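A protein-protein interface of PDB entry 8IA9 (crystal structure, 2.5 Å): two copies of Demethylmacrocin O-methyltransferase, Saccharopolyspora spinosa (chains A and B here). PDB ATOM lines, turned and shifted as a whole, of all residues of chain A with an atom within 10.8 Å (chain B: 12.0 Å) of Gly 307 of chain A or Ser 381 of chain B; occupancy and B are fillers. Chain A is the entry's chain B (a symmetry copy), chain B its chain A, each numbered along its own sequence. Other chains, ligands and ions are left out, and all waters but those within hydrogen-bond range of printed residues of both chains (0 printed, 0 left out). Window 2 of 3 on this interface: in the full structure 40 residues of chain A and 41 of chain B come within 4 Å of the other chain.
No position is printed for both chains. Of the 9 pairs that touch across the chains among the printed residues, none has its exchanged pair printed and touching as well.
Among the printed residues, merely in contact across the chains: Gly 307 of chain A with Arg 380 of chain B, Trp 301 of chain A with Val 374 of chain B, Ala 312 of chain A with Pro 338 of chain B, Tyr 304 of chain A with Glu 336 of chain B, Trp 301 of chain A with Arg 380 of chain B, Trp 301 of chain A with Glu 336 of chain B, Gln 313 of chain A with Pro 338 of chain B, Gly 307 of chain A with Ser 381 of chain B and Trp 301 of chain A with Pro 379 of chain B.
Printed residues of chain B that touch a printed residue of chain A: Glu 336, Pro 338, Val 374, Pro 379, Arg 380 and Ser 381. Hydrophobic or aromatic side chains of chain B that line the printed part of chain A: Pro 338 and Val 374. Of the 20 printed residues of chain A, 5 touch a printed residue of chain B. Hydrophobic or aromatic side chains of chain A that line the printed part of chain B: Trp 301 and Tyr 304. Among the printed residues, 9 pairs touch across the chains.
No residue of chain B comes within 4 Å of Ala 305 of chain A. No residue of chain B comes within 4 Å of Pro 306 of chain A. Gly 307 of chain A touches just these residues of chain B: Arg 380 (3.3 Å) and Ser 381 (3.9 Å). No residue of chain B comes within 4 Å of Gly 309 of chain A. No residue of chain B comes within 4 Å of Gly 310 of chain A. Of the printed residues of chain B, Ala 312 of chain A touches Pro 338. Of the printed residues of chain B, Gln 313 of chain A touches Pro 338 (3.9 Å). Of the printed residues of chain A, Pro 379 of chain B touches Trp 301. Of the printed residues of chain A, Arg 380 of chain B touches Trp 301 and Gly 307. Ser 381 of chain B touches one residue of chain A. No residue of chain A comes within 4 Å of Leu 382 of chain B. No residue of chain A comes within 4 Å of Asp 384 of chain B. No residue of chain A comes within 4 Å of Ile 385 of chain B. The nearest residue of chain B that does not touch Gly 307 of chain A is Leu 382 of chain B (5.2 Å). The nearest printed residue of chain A that does not touch Val 374 of chain B is Thr 302 of chain A (6.5 Å).
The side-chain carboxylate (OE1) of Glu 336 of chain B lies within hydrogen-bond range of the backbone NH (N) of Val 374 of chain B (2.8 Å). The backbone carbonyl oxygen of Val 374 of chain B sits at hydrogen-bond distance from the guanidinium group of Arg 380 of chain B, at 3.2 Å. The backbone NH (N) of Arg 380 of chain B is in hydrogen-bond range of the side-chain carboxylate (OD2) of Asp 384 of chain B. The backbone NH (N) of Asp 383 of chain B sits close to the side-chain hydroxyl (OG) of Ser 381 of chain B, 3.4 Å away.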
ATOM      1  N   SER A 272      -6.145  -2.839  -2.383  1.00  0.00           N
ATOM      2  CA  SER A 272      -7.469  -2.754  -1.706  1.00  0.00           C
ATOM      3  C   SER A 272      -8.281  -4.035  -1.956  1.00  0.00           C
ATOM      4  O   SER A 272      -8.927  -4.515  -0.997  1.00  0.00           O
ATOM      5  CB  SER A 272      -8.230  -1.530  -2.162  1.00  0.00           C
ATOM      6  OG  SER A 272      -8.510  -1.582  -3.556  1.00  0.00           O
ATOM      7  N   HIS A 273      -8.130  -4.632  -3.147  1.00  0.00           N
ATOM      8  CA  HIS A 273      -8.888  -5.812  -3.645  1.00  0.00           C
ATOM      9  C   HIS A 273     -10.317  -5.382  -4.002  1.00  0.00           C
ATOM     10  O   HIS A 273     -11.201  -6.253  -4.146  1.00  0.00           O
ATOM     11  CB  HIS A 273      -8.862  -6.960  -2.631  1.00  0.00           C
ATOM     12  CG  HIS A 273      -7.506  -7.275  -2.106  1.00  0.00           C
ATOM     13  ND1 HIS A 273      -7.255  -7.427  -0.751  1.00  0.00           N
ATOM     14  CD2 HIS A 273      -6.326  -7.467  -2.739  1.00  0.00           C
ATOM     15  CE1 HIS A 273      -5.979  -7.721  -0.573  1.00  0.00           C
ATOM     16  NE2 HIS A 273      -5.383  -7.723  -1.775  1.00  0.00           N
ATOM     17  N   ILE A 274     -10.557  -4.072  -4.049  1.00  0.00           N
ATOM     18  CA  ILE A 274     -11.820  -3.481  -4.578  1.00  0.00           C
ATOM     19  C   ILE A 274     -11.856  -3.755  -6.086  1.00  0.00           C
ATOM     20  O   ILE A 274     -10.840  -3.494  -6.749  1.00  0.00           O
ATOM     21  CB  ILE A 274     -11.907  -1.982  -4.234  1.00  0.00           C
ATOM     22  CG1 ILE A 274     -11.996  -1.762  -2.720  1.00  0.00           C
ATOM     23  CG2 ILE A 274     -13.062  -1.325  -4.975  1.00  0.00           C
ATOM     24  CD1 ILE A 274     -11.819  -0.323  -2.298  1.00  0.00           C
ATOM     25  N   ASN A 275     -12.854  -4.521  -6.527  1.00  0.00           N
ATOM     26  CA  ASN A 275     -12.986  -5.037  -7.914  1.00  0.00           C
ATOM     27  C   ASN A 275     -12.707  -3.911  -8.914  1.00  0.00           C
ATOM     28  O   ASN A 275     -11.879  -4.133  -9.818  1.00  0.00           O
ATOM     29  CB  ASN A 275     -14.348  -5.702  -8.147  1.00  0.00           C
ATOM     30  CG  ASN A 275     -14.477  -7.057  -7.473  1.00  0.00           C
ATOM     31  OD1 ASN A 275     -14.433  -8.090  -8.135  1.00  0.00           O
ATOM     32  ND2 ASN A 275     -14.648  -7.066  -6.164  1.00  0.00           N
ATOM     33  N   GLY A 276     -13.300  -2.728  -8.714  1.00  0.00           N
ATOM     34  CA  GLY A 276     -13.118  -1.555  -9.594  1.00  0.00           C
ATOM     35  C   GLY A 276     -11.653  -1.158  -9.723  1.00  0.00           C
ATOM     36  O   GLY A 276     -11.214  -0.814 -10.840  1.00  0.00           O
ATOM     37  N   HIS A 277     -10.960  -1.055  -8.590  1.00  0.00           N
ATOM     38  CA  HIS A 277      -9.514  -0.735  -8.502  1.00  0.00           C
ATOM     39  C   HIS A 277      -8.704  -1.791  -9.276  1.00  0.00           C
ATOM     40  O   HIS A 277      -7.784  -1.397 -10.046  1.00  0.00           O
ATOM     41  CB  HIS A 277      -9.117  -0.631  -7.024  1.00  0.00           C
ATOM     42  CG  HIS A 277      -9.805   0.474  -6.287  1.00  0.00           C
ATOM     43  ND1 HIS A 277      -9.323   0.976  -5.090  1.00  0.00           N
ATOM     44  CD2 HIS A 277     -10.900   1.212  -6.594  1.00  0.00           C
ATOM     45  CE1 HIS A 277     -10.106   1.956  -4.683  1.00  0.00           C
ATOM     46  NE2 HIS A 277     -11.060   2.142  -5.608  1.00  0.00           N
ATOM     47  N   TRP A 301     -10.849 -13.696  -4.225  1.00  0.00           N
ATOM     48  CA  TRP A 301     -12.041 -14.001  -3.386  1.00  0.00           C
ATOM     49  C   TRP A 301     -12.974 -12.781  -3.269  1.00  0.00           C
ATOM     50  O   TRP A 301     -14.195 -12.984  -3.298  1.00  0.00           O
ATOM     51  CB  TRP A 301     -11.604 -14.508  -2.008  1.00  0.00           C
ATOM     52  CG  TRP A 301     -10.877 -13.494  -1.175  1.00  0.00           C
ATOM     53  CD1 TRP A 301      -9.529 -13.279  -1.125  1.00  0.00           C
ATOM     54  CD2 TRP A 301     -11.457 -12.619  -0.192  1.00  0.00           C
ATOM     55  NE1 TRP A 301      -9.233 -12.355  -0.164  1.00  0.00           N
ATOM     56  CE2 TRP A 301     -10.397 -11.886   0.381  1.00  0.00           C
ATOM     57  CE3 TRP A 301     -12.766 -12.354   0.225  1.00  0.00           C
ATOM     58  CZ2 TRP A 301     -10.602 -10.934   1.378  1.00  0.00           C
ATOM     59  CZ3 TRP A 301     -12.965 -11.438   1.234  1.00  0.00           C
ATOM     60  CH2 TRP A 301     -11.899 -10.718   1.781  1.00  0.00           C
ATOM     61  N   THR A 302     -12.428 -11.565  -3.198  1.00  0.00           N
ATOM     62  CA  THR A 302     -13.204 -10.308  -3.047  1.00  0.00           C
ATOM     63  C   THR A 302     -14.196 -10.164  -4.205  1.00  0.00           C
ATOM     64  O   THR A 302     -15.163  -9.387  -4.047  1.00  0.00           O
ATOM     65  CB  THR A 302     -12.297  -9.081  -2.974  1.00  0.00           C
ATOM     66  OG1 THR A 302     -11.701  -8.935  -4.263  1.00  0.00           O
ATOM     67  CG2 THR A 302     -11.261  -9.208  -1.882  1.00  0.00           C
ATOM     68  N   THR A 303     -13.989 -10.917  -5.290  1.00  0.00           N
ATOM     69  CA  THR A 303     -14.967 -11.077  -6.396  1.00  0.00           C
ATOM     70  C   THR A 303     -16.385 -11.248  -5.825  1.00  0.00           C
ATOM     71  O   THR A 303     -17.338 -10.685  -6.430  1.00  0.00           O
ATOM     72  CB  THR A 303     -14.659 -12.306  -7.262  1.00  0.00           C
ATOM     73  OG1 THR A 303     -13.534 -12.021  -8.099  1.00  0.00           O
ATOM     74  CG2 THR A 303     -15.844 -12.715  -8.111  1.00  0.00           C
ATOM     75  N   TYR A 304     -16.504 -11.935  -4.678  1.00  0.00           N
ATOM     76  CA  TYR A 304     -17.786 -12.434  -4.102  1.00  0.00           C
ATOM     77  C   TYR A 304     -18.200 -11.658  -2.840  1.00  0.00           C
ATOM     78  O   TYR A 304     -19.228 -12.019  -2.230  1.00  0.00           O
ATOM     79  CB  TYR A 304     -17.658 -13.932  -3.810  1.00  0.00           C
ATOM     80  CG  TYR A 304     -17.346 -14.765  -5.026  1.00  0.00           C
ATOM     81  CD1 TYR A 304     -18.277 -14.914  -6.041  1.00  0.00           C
ATOM     82  CD2 TYR A 304     -16.095 -15.337  -5.206  1.00  0.00           C
ATOM     83  CE1 TYR A 304     -18.012 -15.697  -7.154  1.00  0.00           C
ATOM     84  CE2 TYR A 304     -15.793 -16.073  -6.341  1.00  0.00           C
ATOM     85  CZ  TYR A 304     -16.761 -16.280  -7.307  1.00  0.00           C
ATOM     86  OH  TYR A 304     -16.462 -16.996  -8.435  1.00  0.00           O
ATOM     87  N   ALA A 305     -17.451 -10.614  -2.475  1.00  0.00           N
ATOM     88  CA  ALA A 305     -17.651  -9.815  -1.243  1.00  0.00           C
ATOM     89  C   ALA A 305     -18.238  -8.453  -1.600  1.00  0.00           C
ATOM     90  O   ALA A 305     -17.561  -7.612  -2.185  1.00  0.00           O
ATOM     91  CB  ALA A 305     -16.336  -9.694  -0.511  1.00  0.00           C
ATOM     92  N   PRO A 306     -19.501  -8.171  -1.207  1.00  0.00           N
ATOM     93  CA  PRO A 306     -20.156  -6.905  -1.537  1.00  0.00           C
ATOM     94  C   PRO A 306     -19.384  -5.680  -1.028  1.00  0.00           C
ATOM     95  O   PRO A 306     -19.384  -4.671  -1.702  1.00  0.00           O
ATOM     96  CB  PRO A 306     -21.527  -6.983  -0.839  1.00  0.00           C
ATOM     97  CG  PRO A 306     -21.739  -8.453  -0.568  1.00  0.00           C
ATOM     98  CD  PRO A 306     -20.352  -9.039  -0.380  1.00  0.00           C
ATOM     99  N   GLY A 307     -18.676  -5.829   0.097  1.00  0.00           N
ATOM    100  CA  GLY A 307     -17.880  -4.756   0.729  1.00  0.00           C
ATOM    101  C   GLY A 307     -16.661  -4.367  -0.093  1.00  0.00           C
ATOM    102  O   GLY A 307     -15.954  -3.427   0.317  1.00  0.00           O
ATOM    103  N   PHE A 308     -16.362  -5.119  -1.156  1.00  0.00           N
ATOM    104  CA  PHE A 308     -15.213  -4.870  -2.066  1.00  0.00           C
ATOM    105  C   PHE A 308     -15.726  -4.590  -3.480  1.00  0.00           C
ATOM    106  O   PHE A 308     -14.921  -4.612  -4.432  1.00  0.00           O
ATOM    107  CB  PHE A 308     -14.246  -6.056  -2.066  1.00  0.00           C
ATOM    108  CG  PHE A 308     -13.385  -6.168  -0.833  1.00  0.00           C
ATOM    109  CD1 PHE A 308     -12.194  -5.463  -0.729  1.00  0.00           C
ATOM    110  CD2 PHE A 308     -13.753  -6.994   0.220  1.00  0.00           C
ATOM    111  CE1 PHE A 308     -11.397  -5.578   0.400  1.00  0.00           C
ATOM    112  CE2 PHE A 308     -12.941  -7.123   1.339  1.00  0.00           C
ATOM    113  CZ  PHE A 308     -11.772  -6.401   1.435  1.00  0.00           C
ATOM    114  N   GLY A 309     -17.007  -4.233  -3.599  1.00  0.00           N
ATOM    115  CA  GLY A 309     -17.657  -3.935  -4.890  1.00  0.00           C
ATOM    116  C   GLY A 309     -17.951  -5.218  -5.638  1.00  0.00           C
ATOM    117  O   GLY A 309     -18.181  -5.145  -6.864  1.00  0.00           O
ATOM    118  N   GLY A 310     -17.879  -6.351  -4.926  1.00  0.00           N
ATOM    119  CA  GLY A 310     -18.191  -7.696  -5.444  1.00  0.00           C
ATOM    120  C   GLY A 310     -19.667  -8.013  -5.282  1.00  0.00           C
ATOM    121  O   GLY A 310     -20.392  -7.115  -4.810  1.00  0.00           O
ATOM    122  N   GLN A 311     -20.124  -9.103  -5.907  1.00  0.00           N
ATOM    123  CA  GLN A 311     -21.498  -9.662  -5.756  1.00  0.00           C
ATOM    124  C   GLN A 311     -21.402 -11.076  -5.169  1.00  0.00           C
ATOM    125  O   GLN A 311     -20.626 -11.900  -5.712  1.00  0.00           O
ATOM    126  CB  GLN A 311     -22.238  -9.728  -7.096  1.00  0.00           C
ATOM    127  CG  GLN A 311     -22.200  -8.434  -7.894  1.00  0.00           C
ATOM    128  CD  GLN A 311     -23.083  -7.348  -7.334  1.00  0.00           C
ATOM    129  OE1 GLN A 311     -23.002  -6.192  -7.739  1.00  0.00           O
ATOM    130  NE2 GLN A 311     -23.922  -7.704  -6.378  1.00  0.00           N
ATOM    131  N   ALA A 312     -22.228 -11.365  -4.164  1.00  0.00           N
ATOM    132  CA  ALA A 312     -22.338 -12.688  -3.513  1.00  0.00           C
ATOM    133  C   ALA A 312     -23.281 -13.571  -4.334  1.00  0.00           C
ATOM    134  O   ALA A 312     -24.182 -14.155  -3.742  1.00  0.00           O
ATOM    135  CB  ALA A 312     -22.802 -12.546  -2.085  1.00  0.00           C
ATOM    136  N   GLN A 313     -22.950 -13.786  -5.610  1.00  0.00           N
ATOM    137  CA  GLN A 313     -23.651 -14.718  -6.529  1.00  0.00           C
ATOM    138  C   GLN A 313     -22.610 -15.554  -7.296  1.00  0.00           C
ATOM    139  O   GLN A 313     -21.440 -15.152  -7.350  1.00  0.00           O
ATOM    140  CB  GLN A 313     -24.542 -13.919  -7.477  1.00  0.00           C
ATOM    141  CG  GLN A 313     -23.751 -13.063  -8.454  1.00  0.00           C
ATOM    142  CD  GLN A 313     -24.643 -12.249  -9.359  1.00  0.00           C
ATOM    143  OE1 GLN A 313     -24.811 -12.553 -10.538  1.00  0.00           O
ATOM    144  NE2 GLN A 313     -25.251 -11.219  -8.798  1.00  0.00           N
ATOM    145  N   THR A 320     -16.668  -8.024 -11.730  1.00  0.00           N
ATOM    146  CA  THR A 320     -15.942  -8.641 -10.588  1.00  0.00           C
ATOM    147  C   THR A 320     -14.744  -9.407 -11.152  1.00  0.00           C
ATOM    148  O   THR A 320     -14.767  -9.756 -12.343  1.00  0.00           O
ATOM    149  CB  THR A 320     -16.868  -9.508  -9.725  1.00  0.00           C
ATOM    150  OG1 THR A 320     -17.227 -10.667 -10.476  1.00  0.00           O
ATOM    151  CG2 THR A 320     -18.113  -8.763  -9.290  1.00  0.00           C
ATOM    152  N   GLU B 336     -14.431 -19.973  -2.029  1.00  0.00           N
ATOM    153  CA  GLU B 336     -14.595 -18.510  -1.775  1.00  0.00           C
ATOM    154  C   GLU B 336     -15.987 -18.069  -2.221  1.00  0.00           C
ATOM    155  O   GLU B 336     -16.296 -16.889  -2.025  1.00  0.00           O
ATOM    156  CB  GLU B 336     -13.524 -17.689  -2.501  1.00  0.00           C
ATOM    157  CG  GLU B 336     -12.113 -18.243  -2.361  1.00  0.00           C
ATOM    158  CD  GLU B 336     -11.535 -18.190  -0.955  1.00  0.00           C
ATOM    159  OE1 GLU B 336     -12.226 -17.649  -0.060  1.00  0.00           O
ATOM    160  OE2 GLU B 336     -10.381 -18.660  -0.768  1.00  0.00           O
ATOM    161  N   PRO B 338     -20.072 -17.930  -2.354  1.00  0.00           N
ATOM    162  CA  PRO B 338     -21.140 -18.049  -1.363  1.00  0.00           C
ATOM    163  C   PRO B 338     -22.035 -19.273  -1.625  1.00  0.00           C
ATOM    164  O   PRO B 338     -22.330 -19.551  -2.778  1.00  0.00           O
ATOM    165  CB  PRO B 338     -21.925 -16.754  -1.601  1.00  0.00           C
ATOM    166  CG  PRO B 338     -21.840 -16.570  -3.103  1.00  0.00           C
ATOM    167  CD  PRO B 338     -20.463 -17.082  -3.487  1.00  0.00           C
ATOM    168  N   VAL B 374     -11.191 -18.147   2.444  1.00  0.00           N
ATOM    169  CA  VAL B 374     -10.701 -17.056   3.332  1.00  0.00           C
ATOM    170  C   VAL B 374     -11.463 -17.153   4.646  1.00  0.00           C
ATOM    171  O   VAL B 374     -12.678 -16.996   4.668  1.00  0.00           O
ATOM    172  CB  VAL B 374     -10.855 -15.670   2.679  1.00  0.00           C
ATOM    173  CG1 VAL B 374     -10.370 -14.572   3.608  1.00  0.00           C
ATOM    174  CG2 VAL B 374     -10.146 -15.589   1.339  1.00  0.00           C
ATOM    175  N   PRO B 375     -10.762 -17.358   5.782  1.00  0.00           N
ATOM    176  CA  PRO B 375     -11.414 -17.483   7.085  1.00  0.00           C
ATOM    177  C   PRO B 375     -12.487 -16.413   7.340  1.00  0.00           C
ATOM    178  O   PRO B 375     -12.336 -15.290   6.875  1.00  0.00           O
ATOM    179  CB  PRO B 375     -10.268 -17.316   8.086  1.00  0.00           C
ATOM    180  CG  PRO B 375      -9.047 -17.774   7.315  1.00  0.00           C
ATOM    181  CD  PRO B 375      -9.295 -17.342   5.883  1.00  0.00           C
ATOM    182  N   ALA B 376     -13.508 -16.774   8.120  1.00  0.00           N
ATOM    183  CA  ALA B 376     -14.699 -15.941   8.389  1.00  0.00           C
ATOM    184  C   ALA B 376     -14.314 -14.754   9.275  1.00  0.00           C
ATOM    185  O   ALA B 376     -15.139 -13.817   9.382  1.00  0.00           O
ATOM    186  CB  ALA B 376     -15.780 -16.777   9.023  1.00  0.00           C
ATOM    187  N   TRP B 377     -13.142 -14.813   9.918  1.00  0.00           N
ATOM    188  CA  TRP B 377     -12.624 -13.734  10.805  1.00  0.00           C
ATOM    189  C   TRP B 377     -11.873 -12.661   9.998  1.00  0.00           C
ATOM    190  O   TRP B 377     -11.392 -11.690  10.614  1.00  0.00           O
ATOM    191  CB  TRP B 377     -11.750 -14.303  11.931  1.00  0.00           C
ATOM    192  CG  TRP B 377     -10.633 -15.197  11.487  1.00  0.00           C
ATOM    193  CD1 TRP B 377     -10.590 -16.557  11.576  1.00  0.00           C
ATOM    194  CD2 TRP B 377      -9.324 -14.783  11.051  1.00  0.00           C
ATOM    195  NE1 TRP B 377      -9.376 -17.021  11.143  1.00  0.00           N
ATOM    196  CE2 TRP B 377      -8.576 -15.959  10.821  1.00  0.00           C
ATOM    197  CE3 TRP B 377      -8.721 -13.542  10.809  1.00  0.00           C
ATOM    198  CZ2 TRP B 377      -7.263 -15.926  10.357  1.00  0.00           C
ATOM    199  CZ3 TRP B 377      -7.433 -13.513  10.323  1.00  0.00           C
ATOM    200  CH2 TRP B 377      -6.724 -14.690  10.076  1.00  0.00           C
ATOM    201  N   VAL B 378     -11.737 -12.824   8.680  1.00  0.00           N
ATOM    202  CA  VAL B 378     -11.138 -11.775   7.801  1.00  0.00           C
ATOM    203  C   VAL B 378     -12.227 -10.768   7.440  1.00  0.00           C
ATOM    204  O   VAL B 378     -13.289 -11.142   6.946  1.00  0.00           O
ATOM    205  CB  VAL B 378     -10.479 -12.378   6.548  1.00  0.00           C
ATOM    206  CG1 VAL B 378     -10.204 -11.323   5.490  1.00  0.00           C
ATOM    207  CG2 VAL B 378      -9.206 -13.134   6.900  1.00  0.00           C
ATOM    208  N   PRO B 379     -12.001  -9.460   7.699  1.00  0.00           N
ATOM    209  CA  PRO B 379     -13.000  -8.425   7.418  1.00  0.00           C
ATOM    210  C   PRO B 379     -13.486  -8.424   5.958  1.00  0.00           C
ATOM    211  O   PRO B 379     -12.671  -8.603   5.067  1.00  0.00           O
ATOM    212  CB  PRO B 379     -12.258  -7.123   7.743  1.00  0.00           C
ATOM    213  CG  PRO B 379     -11.202  -7.535   8.745  1.00  0.00           C
ATOM    214  CD  PRO B 379     -10.781  -8.924   8.319  1.00  0.00           C
ATOM    215  N   ARG B 380     -14.773  -8.131   5.745  1.00  0.00           N
ATOM    216  CA  ARG B 380     -15.455  -8.216   4.423  1.00  0.00           C
ATOM    217  C   ARG B 380     -15.969  -6.842   3.986  1.00  0.00           C
ATOM    218  O   ARG B 380     -16.832  -6.830   3.085  1.00  0.00           O
ATOM    219  CB  ARG B 380     -16.663  -9.154   4.496  1.00  0.00           C
ATOM    220  CG  ARG B 380     -16.333 -10.574   4.930  1.00  0.00           C
ATOM    221  CD  ARG B 380     -16.298 -11.507   3.748  1.00  0.00           C
ATOM    222  NE  ARG B 380     -15.441 -12.643   4.021  1.00  0.00           N
ATOM    223  CZ  ARG B 380     -15.260 -13.646   3.177  1.00  0.00           C
ATOM    224  NH1 ARG B 380     -15.900 -13.627   2.017  1.00  0.00           N
ATOM    225  NH2 ARG B 380     -14.478 -14.668   3.512  1.00  0.00           N
ATOM    226  N   SER B 381     -15.558  -5.763   4.670  1.00  0.00           N
ATOM    227  CA  SER B 381     -16.080  -4.379   4.485  1.00  0.00           C
ATOM    228  C   SER B 381     -15.426  -3.415   5.483  1.00  0.00           C
ATOM    229  O   SER B 381     -14.606  -3.880   6.293  1.00  0.00           O
ATOM    230  CB  SER B 381     -17.584  -4.369   4.638  1.00  0.00           C
ATOM    231  OG  SER B 381     -17.975  -5.073   5.808  1.00  0.00           O
ATOM    232  N   LEU B 382     -15.748  -2.116   5.388  1.00  0.00           N
ATOM    233  CA  LEU B 382     -15.438  -1.090   6.427  1.00  0.00           C
ATOM    234  C   LEU B 382     -16.428  -1.270   7.587  1.00  0.00           C
ATOM    235  O   LEU B 382     -16.206  -0.670   8.662  1.00  0.00           O
ATOM    236  CB  LEU B 382     -15.527   0.328   5.843  1.00  0.00           C
ATOM    237  CG  LEU B 382     -14.253   0.883   5.199  1.00  0.00           C
ATOM    238  CD1 LEU B 382     -14.382   2.378   4.942  1.00  0.00           C
ATOM    239  CD2 LEU B 382     -13.025   0.602   6.056  1.00  0.00           C
ATOM    240  N   ASP B 383     -17.496  -2.043   7.352  1.00  0.00           N
ATOM    241  CA  ASP B 383     -18.527  -2.415   8.362  1.00  0.00           C
ATOM    242  C   ASP B 383     -17.833  -3.203   9.483  1.00  0.00           C
ATOM    243  O   ASP B 383     -18.035  -2.849  10.662  1.00  0.00           O
ATOM    244  CB  ASP B 383     -19.661  -3.221   7.710  1.00  0.00           C
ATOM    245  CG  ASP B 383     -21.053  -2.958   8.270  1.00  0.00           C
ATOM    246  OD1 ASP B 383     -21.306  -1.813   8.694  1.00  0.00           O
ATOM    247  OD2 ASP B 383     -21.907  -3.869   8.183  1.00  0.00           O
ATOM    248  N   ASP B 384     -16.863  -4.047   9.106  1.00  0.00           N
ATOM    249  CA  ASP B 384     -16.120  -4.967  10.012  1.00  0.00           C
ATOM    250  C   ASP B 384     -14.823  -4.300  10.497  1.00  0.00           C
ATOM    251  O   ASP B 384     -14.362  -4.653  11.602  1.00  0.00           O
ATOM    252  CB  ASP B 384     -15.805  -6.295   9.313  1.00  0.00           C
ATOM    253  CG  ASP B 384     -17.024  -7.129   8.954  1.00  0.00           C
ATOM    254  OD1 ASP B 384     -18.133  -6.775   9.405  1.00  0.00           O
ATOM    255  OD2 ASP B 384     -16.849  -8.141   8.241  1.00  0.00           O
ATOM    256  N   ILE B 385     -14.203  -3.459   9.660  1.00  0.00           N
ATOM    257  CA  ILE B 385     -12.934  -2.728   9.967  1.00  0.00           C
ATOM    258  C   ILE B 385     -13.172  -1.760  11.139  1.00  0.00           C
ATOM    259  O   ILE B 385     -12.277  -1.669  12.002  1.00  0.00           O
ATOM    260  CB  ILE B 385     -12.396  -1.994   8.717  1.00  0.00           C
ATOM    261  CG1 ILE B 385     -11.903  -2.964   7.636  1.00  0.00           C
ATOM    262  CG2 ILE B 385     -11.314  -0.991   9.097  1.00  0.00           C
ATOM    263  CD1 ILE B 385     -10.529  -3.538   7.894  1.00  0.00           C
ATOM    264  N   LEU B 386     -14.371  -1.166  11.230  1.00  0.00           N
ATOM    265  CA  LEU B 386     -14.733  -0.127  12.241  1.00  0.00           C
ATOM    266  C   LEU B 386     -14.894  -0.762  13.630  1.00  0.00           C
ATOM    267  O   LEU B 386     -14.822  -0.011  14.623  1.00  0.00           O
ATOM    268  CB  LEU B 386     -16.017   0.596  11.809  1.00  0.00           C
ATOM    269  CG  LEU B 386     -16.478   1.739  12.719  1.00  0.00           C
ATOM    270  CD1 LEU B 386     -17.236   2.802  11.932  1.00  0.00           C
ATOM    271  CD2 LEU B 386     -17.333   1.225  13.869  1.00  0.00           C
ATOM    272  N   HIS B 387     -15.185  -2.067  13.695  1.00  0.00           N
ATOM    273  CA  HIS B 387     -15.287  -2.856  14.956  1.00  0.00           C
ATOM    274  C   HIS B 387     -13.923  -3.484  15.268  1.00  0.00           C
ATOM    275  O   HIS B 387     -13.643  -3.935  16.375  1.00  0.00           O
ATOM    276  CB  HIS B 387     -16.405  -3.910  14.859  1.00  0.00           C
ATOM    277  CG  HIS B 387     -17.779  -3.342  14.704  1.00  0.00           C
ATOM    278  ND1 HIS B 387     -18.392  -2.594  15.695  1.00  0.00           N
ATOM    279  CD2 HIS B 387     -18.699  -3.486  13.722  1.00  0.00           C
ATOM    280  CE1 HIS B 387     -19.603  -2.250  15.302  1.00  0.00           C
ATOM    281  NE2 HIS B 387     -19.814  -2.782  14.093  1.00  0.00           N
